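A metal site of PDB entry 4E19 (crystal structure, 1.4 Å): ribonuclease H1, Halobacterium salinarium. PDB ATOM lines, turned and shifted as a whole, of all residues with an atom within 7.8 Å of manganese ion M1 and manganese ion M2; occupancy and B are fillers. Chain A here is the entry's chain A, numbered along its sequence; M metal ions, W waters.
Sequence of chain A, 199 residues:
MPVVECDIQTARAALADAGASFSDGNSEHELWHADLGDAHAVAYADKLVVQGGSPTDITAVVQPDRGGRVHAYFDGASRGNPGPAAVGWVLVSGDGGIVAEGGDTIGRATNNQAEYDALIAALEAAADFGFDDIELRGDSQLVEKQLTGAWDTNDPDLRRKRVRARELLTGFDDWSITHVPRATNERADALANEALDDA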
ATOM      1  N   PHE A  74     -20.899 -28.992  -3.754  1.00  0.00           N
ATOM      2  CA  PHE A  74     -19.592 -29.288  -3.235  1.00  0.00           C
ATOM      3  C   PHE A  74     -18.615 -29.131  -4.345  1.00  0.00           C
ATOM      4  O   PHE A  74     -18.902 -29.499  -5.511  1.00  0.00           O
ATOM      5  CB  PHE A  74     -19.535 -30.641  -2.573  1.00  0.00           C
ATOM      6  CG  PHE A  74     -19.754 -31.809  -3.492  1.00  0.00           C
ATOM      7  CD1 PHE A  74     -18.678 -32.425  -4.046  1.00  0.00           C
ATOM      8  CD2 PHE A  74     -21.037 -32.242  -3.745  1.00  0.00           C
ATOM      9  CE1 PHE A  74     -18.865 -33.545  -4.877  1.00  0.00           C
ATOM     10  CE2 PHE A  74     -21.212 -33.329  -4.584  1.00  0.00           C
ATOM     11  CZ  PHE A  74     -20.178 -33.976  -5.151  1.00  0.00           C
ATOM     12  N   ASP A  75     -17.345 -28.800  -4.017  1.00  0.00           N
ATOM     13  CA  ASP A  75     -16.233 -28.768  -5.027  1.00  0.00           C
ATOM     14  C   ASP A  75     -14.934 -28.881  -4.350  1.00  0.00           C
ATOM     15  O   ASP A  75     -14.671 -28.277  -3.289  1.00  0.00           O
ATOM     16  CB  ASP A  75     -16.270 -27.527  -5.845  1.00  0.00           C
ATOM     17  CG  ASP A  75     -15.463 -27.681  -7.039  1.00  0.00           C
ATOM     18  OD1 ASP A  75     -15.368 -28.786  -7.699  1.00  0.00           O
ATOM     19  OD2 ASP A  75     -14.804 -26.655  -7.468  1.00  0.00           O
ATOM     20  N   GLY A  76     -14.089 -29.717  -4.953  1.00  0.00           N
ATOM     21  CA  GLY A  76     -12.657 -29.788  -4.566  1.00  0.00           C
ATOM     22  C   GLY A  76     -11.770 -28.883  -5.393  1.00  0.00           C
ATOM     23  O   GLY A  76     -12.084 -28.531  -6.572  1.00  0.00           O
ATOM     24  N   ALA A  77     -10.608 -28.559  -4.831  1.00  0.00           N
ATOM     25  CA  ALA A  77      -9.564 -27.841  -5.604  1.00  0.00           C
ATOM     26  C   ALA A  77      -8.240 -28.485  -5.126  1.00  0.00           C
ATOM     27  O   ALA A  77      -8.025 -28.747  -3.956  1.00  0.00           O
ATOM     28  CB  ALA A  77      -9.534 -26.332  -5.367  1.00  0.00           C
ATOM     29  N   SER A  78      -7.338 -28.713  -6.081  1.00  0.00           N
ATOM     30  CA  SER A  78      -6.002 -29.203  -5.728  1.00  0.00           C
ATOM     31  C   SER A  78      -4.966 -28.723  -6.728  1.00  0.00           C
ATOM     32  O   SER A  78      -5.207 -28.656  -7.873  1.00  0.00           O
ATOM     33  CB  SER A  78      -5.928 -30.680  -5.731  1.00  0.00           C
ATOM     34  OG  SER A  78      -4.604 -31.111  -5.504  1.00  0.00           O
ATOM     35  N   ASN A 111      -6.629 -34.068  -6.680  1.00  0.00           N
ATOM     36  CA  ASN A 111      -7.924 -33.620  -7.194  1.00  0.00           C
ATOM     37  C   ASN A 111      -9.072 -34.554  -6.779  1.00  0.00           C
ATOM     38  O   ASN A 111     -10.122 -34.022  -6.296  1.00  0.00           O
ATOM     39  CB  ASN A 111      -7.823 -33.520  -8.740  1.00  0.00           C
ATOM     40  CG  ASN A 111      -7.340 -34.853  -9.477  1.00  0.00           C
ATOM     41  OD1 ASN A 111      -6.884 -35.901  -8.912  1.00  0.00           O
ATOM     42  ND2 ASN A 111      -7.323 -34.691 -10.836  1.00  0.00           N
ATOM     43  N   ALA A 114      -9.812 -34.322  -3.121  1.00  0.00           N
ATOM     44  CA  ALA A 114     -10.410 -33.080  -2.671  1.00  0.00           C
ATOM     45  C   ALA A 114     -11.892 -33.018  -3.030  1.00  0.00           C
ATOM     46  O   ALA A 114     -12.719 -32.542  -2.242  1.00  0.00           O
ATOM     47  CB  ALA A 114      -9.671 -31.893  -3.227  1.00  0.00           C
ATOM     48  N   GLU A 115     -12.226 -33.507  -4.220  1.00  0.00           N
ATOM     49  CA  GLU A 115     -13.607 -33.536  -4.672  1.00  0.00           C
ATOM     50  C   GLU A 115     -14.444 -34.442  -3.762  1.00  0.00           C
ATOM     51  O   GLU A 115     -15.646 -34.238  -3.597  1.00  0.00           O
ATOM     52  CB  GLU A 115     -13.693 -34.033  -6.117  1.00  0.00           C
ATOM     53  CG  GLU A 115     -13.163 -33.044  -7.140  1.00  0.00           C
ATOM     54  CD  GLU A 115     -14.212 -32.048  -7.599  1.00  0.00           C
ATOM     55  OE1 GLU A 115     -15.178 -31.810  -6.832  1.00  0.00           O
ATOM     56  OE2 GLU A 115     -14.073 -31.503  -8.712  1.00  0.00           O
ATOM     57  N   GLY A 138     -22.651 -31.579  -7.781  1.00  0.00           N
ATOM     58  CA  GLY A 138     -21.187 -31.421  -7.946  1.00  0.00           C
ATOM     59  C   GLY A 138     -20.846 -31.614  -9.408  1.00  0.00           C
ATOM     60  O   GLY A 138     -21.731 -31.821 -10.255  1.00  0.00           O
ATOM     61  N   ASP A 139     -19.592 -31.403  -9.664  1.00  0.00           N
ATOM     62  CA  ASP A 139     -19.145 -31.429 -11.068  1.00  0.00           C
ATOM     63  C   ASP A 139     -18.044 -32.471 -11.218  1.00  0.00           C
ATOM     64  O   ASP A 139     -17.340 -32.483 -12.282  1.00  0.00           O
ATOM     65  CB  ASP A 139     -18.652 -30.032 -11.524  1.00  0.00           C
ATOM     66  CG  ASP A 139     -17.654 -29.418 -10.566  1.00  0.00           C
ATOM     67  OD1 ASP A 139     -16.811 -30.212 -10.085  1.00  0.00           O
ATOM     68  OD2 ASP A 139     -17.613 -28.178 -10.388  1.00  0.00           O
ATOM     69  N   SER A 140     -17.912 -33.428 -10.292  1.00  0.00           N
ATOM     70  CA  SER A 140     -16.914 -34.512 -10.435  1.00  0.00           C
ATOM     71  C   SER A 140     -17.635 -35.811 -10.871  1.00  0.00           C
ATOM     72  O   SER A 140     -18.346 -36.477 -10.068  1.00  0.00           O
ATOM     73  CB  SER A 140     -16.314 -34.766  -9.037  1.00  0.00           C
ATOM     74  OG  SER A 140     -15.557 -35.973  -9.046  1.00  0.00           O
ATOM     75  N   GLN A 141     -17.367 -36.247 -12.072  1.00  0.00           N
ATOM     76  CA  GLN A 141     -17.821 -37.551 -12.556  1.00  0.00           C
ATOM     77  C   GLN A 141     -17.341 -38.618 -11.635  1.00  0.00           C
ATOM     78  O   GLN A 141     -18.141 -39.559 -11.339  1.00  0.00           O
ATOM     79  CB  GLN A 141     -17.280 -37.766 -13.998  1.00  0.00           C
ATOM     80  CG  GLN A 141     -17.703 -39.133 -14.519  1.00  0.00           C
ATOM     81  CD  GLN A 141     -16.908 -39.465 -15.780  1.00  0.00           C
ATOM     82  OE1 GLN A 141     -15.689 -39.461 -15.779  1.00  0.00           O
ATOM     83  NE2 GLN A 141     -17.647 -39.944 -16.820  1.00  0.00           N
ATOM     84  N   VAL A 180     -23.600 -31.085 -12.268  1.00  0.00           N
ATOM     85  CA  VAL A 180     -23.841 -29.730 -12.835  1.00  0.00           C
ATOM     86  C   VAL A 180     -22.440 -29.357 -13.503  1.00  0.00           C
ATOM     87  O   VAL A 180     -21.363 -29.839 -13.079  1.00  0.00           O
ATOM     88  CB  VAL A 180     -24.227 -28.692 -11.818  1.00  0.00           C
ATOM     89  CG1 VAL A 180     -25.610 -29.016 -11.189  1.00  0.00           C
ATOM     90  CG2 VAL A 180     -23.233 -28.592 -10.689  1.00  0.00           C
ATOM     91  N   ARG A 182     -19.213 -27.078 -14.235  1.00  0.00           N
ATOM     92  CA  ARG A 182     -18.567 -26.259 -13.248  1.00  0.00           C
ATOM     93  C   ARG A 182     -19.075 -24.827 -13.159  1.00  0.00           C
ATOM     94  O   ARG A 182     -19.087 -24.229 -12.050  1.00  0.00           O
ATOM     95  CB  ARG A 182     -17.062 -26.356 -13.366  1.00  0.00           C
ATOM     96  CG  ARG A 182     -16.418 -25.904 -14.658  1.00  0.00           C
ATOM     97  CD  ARG A 182     -14.844 -26.260 -14.666  1.00  0.00           C
ATOM     98  NE  ARG A 182     -14.108 -25.645 -13.557  1.00  0.00           N
ATOM     99  CZ  ARG A 182     -13.805 -24.356 -13.493  1.00  0.00           C
ATOM    100  NH1 ARG A 182     -14.199 -23.547 -14.496  1.00  0.00           N
ATOM    101  NH2 ARG A 182     -13.131 -23.860 -12.446  1.00  0.00           N
ATOM    102  N   ASN A 185     -21.691 -24.665 -10.742  1.00  0.00           N
ATOM    103  CA  ASN A 185     -21.066 -24.841  -9.428  1.00  0.00           C
ATOM    104  C   ASN A 185     -20.064 -23.752  -8.948  1.00  0.00           C
ATOM    105  O   ASN A 185     -19.091 -24.041  -8.226  1.00  0.00           O
ATOM    106  CB  ASN A 185     -20.359 -26.201  -9.443  1.00  0.00           C
ATOM    107  CG  ASN A 185     -20.234 -26.836  -8.079  1.00  0.00           C
ATOM    108  OD1 ASN A 185     -20.977 -26.527  -7.102  1.00  0.00           O
ATOM    109  ND2 ASN A 185     -19.239 -27.794  -7.911  1.00  0.00           N
ATOM    110  N   GLU A 186     -20.285 -22.587  -9.553  1.00  0.00           N
ATOM    111  CA  GLU A 186     -19.291 -21.507  -9.334  1.00  0.00           C
ATOM    112  C   GLU A 186     -19.104 -21.101  -7.895  1.00  0.00           C
ATOM    113  O   GLU A 186     -18.012 -20.721  -7.565  1.00  0.00           O
ATOM    114  CB  GLU A 186     -19.672 -20.311 -10.172  1.00  0.00           C
ATOM    115  CG  GLU A 186     -18.859 -18.943 -10.081  1.00  0.00           C
ATOM    116  CD  GLU A 186     -19.583 -17.843 -10.931  1.00  0.00           C
ATOM    117  OE1 GLU A 186     -18.836 -17.025 -11.550  1.00  0.00           O
ATOM    118  OE2 GLU A 186     -20.839 -17.839 -11.043  1.00  0.00           O
ATOM    119  N   ALA A 188     -19.377 -22.954  -4.887  1.00  0.00           N
ATOM    120  CA  ALA A 188     -18.517 -23.870  -4.177  1.00  0.00           C
ATOM    121  C   ALA A 188     -17.098 -23.815  -4.730  1.00  0.00           C
ATOM    122  O   ALA A 188     -16.142 -23.949  -3.980  1.00  0.00           O
ATOM    123  CB  ALA A 188     -19.123 -25.324  -4.289  1.00  0.00           C
ATOM    124  N   ASP A 189     -17.008 -23.718  -6.067  1.00  0.00           N
ATOM    125  CA  ASP A 189     -15.673 -23.624  -6.671  1.00  0.00           C
ATOM    126  C   ASP A 189     -14.924 -22.344  -6.154  1.00  0.00           C
ATOM    127  O   ASP A 189     -13.762 -22.449  -5.853  1.00  0.00           O
ATOM    128  CB  ASP A 189     -15.836 -23.621  -8.199  1.00  0.00           C
ATOM    129  CG  ASP A 189     -14.552 -23.391  -8.916  1.00  0.00           C
ATOM    130  OD1 ASP A 189     -13.860 -24.298  -9.351  1.00  0.00           O
ATOM    131  OD2 ASP A 189     -14.020 -22.218  -8.981  1.00  0.00           O
ATOM    132  N   ALA A 190     -15.604 -21.231  -6.068  1.00  0.00           N
ATOM    133  CA  ALA A 190     -14.992 -19.971  -5.554  1.00  0.00           C
ATOM    134  C   ALA A 190     -14.604 -20.171  -4.060  1.00  0.00           C
ATOM    135  O   ALA A 190     -13.525 -19.817  -3.656  1.00  0.00           O
ATOM    136  CB  ALA A 190     -16.001 -18.844  -5.665  1.00  0.00           C
ATOM    137  N   ALA A 192     -13.718 -22.931  -2.505  1.00  0.00           N
ATOM    138  CA  ALA A 192     -12.527 -23.848  -2.420  1.00  0.00           C
ATOM    139  C   ALA A 192     -11.284 -23.076  -2.942  1.00  0.00           C
ATOM    140  O   ALA A 192     -10.261 -23.203  -2.281  1.00  0.00           O
ATOM    141  CB  ALA A 192     -12.746 -25.100  -3.314  1.00  0.00           C
ATOM    142  N   ASN A 193     -11.392 -22.404  -4.061  1.00  0.00           N
ATOM    143  CA  ASN A 193     -10.245 -21.755  -4.703  1.00  0.00           C
ATOM    144  C   ASN A 193      -9.789 -20.556  -3.901  1.00  0.00           C
ATOM    145  O   ASN A 193      -8.573 -20.331  -3.855  1.00  0.00           O
ATOM    146  CB  ASN A 193     -10.479 -21.512  -6.165  1.00  0.00           C
ATOM    147  CG  ASN A 193     -10.255 -22.827  -6.942  1.00  0.00           C
ATOM    148  OD1 ASN A 193      -9.103 -23.319  -7.126  1.00  0.00           O
ATOM    149  ND2 ASN A 193     -11.337 -23.477  -7.201  1.00  0.00           N
HETATM  150 MN    MN M   1     -14.832 -29.816  -9.414  1.00  0.00          MN
HETATM  151 MN    MN M   2     -13.633 -26.417  -9.261  1.00  0.00          MN
HETATM  152  O   HOH W   1     -12.830 -28.729  -9.178  1.00  0.00           O
HETATM  153  O   HOH W   2     -15.119 -27.428 -10.420  1.00  0.00           O
HETATM  154  O   HOH W   3     -11.735 -26.159  -8.052  1.00  0.00           O
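O of Asp 189 is in hydrogen-bond range of ND2 of Asn 193.
OD2 of Asp 189 lies within salt-bridge range of NH2 of Arg 182, at 3.9 Å.
ND2 of Asn 185 lies within hydrogen-bond range of OD2 of Asp 139 (3.0 Å).
OE1 of Glu 115 is in hydrogen-bond range of N of Gly 76, at 3.0 Å.
Within 4 Å of manganese ion M1: Asp 75, Glu 115 and Asp 139.
Along chain A the residues within 4 Å of manganese ion M1 span positions 75 to 139.
The nearest printed residue that does not touch manganese ion M1 is Gly 76 (4.2 Å).
Gly 76 touches manganese ion M2 (O to MN, 3.8 Å).
Three residues have an atom within 4 Å of manganese ion M2: Asp 75, Gly 76 and Asp 189.
The nearest printed residue that does not touch manganese ion M2 is Arg 182 (4.1 Å).
Manganese ion M1 is bound by OE2 of Glu 115 (2.0 Å), OD1 of Asp 75 (2.1 Å), OD1 of Asp 139 (2.1 Å), water W1 (2.3 Å) and water W2 (2.6 Å).
Manganese ion M1 has five donor atoms within binding distance.
The side-chain carboxylate (OD1) of Asp 189 binds manganese ion M2, at 2.1 Å.
Manganese ion M2 is bound by water W2 (2.1 Å).
Manganese ion M2 is bound by OD2 of Asp 75 (2.2 Å).
Manganese ion M2 is bound by water W3 (2.3 Å).
Water W1 is bound to manganese ion M2, 2.4 Å away.
Manganese ion M2 has five donor atoms within binding distance.
Water W3 bridges O of Gly 76 (2.8 Å) and ND2 of Asn 193 (2.8 Å).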
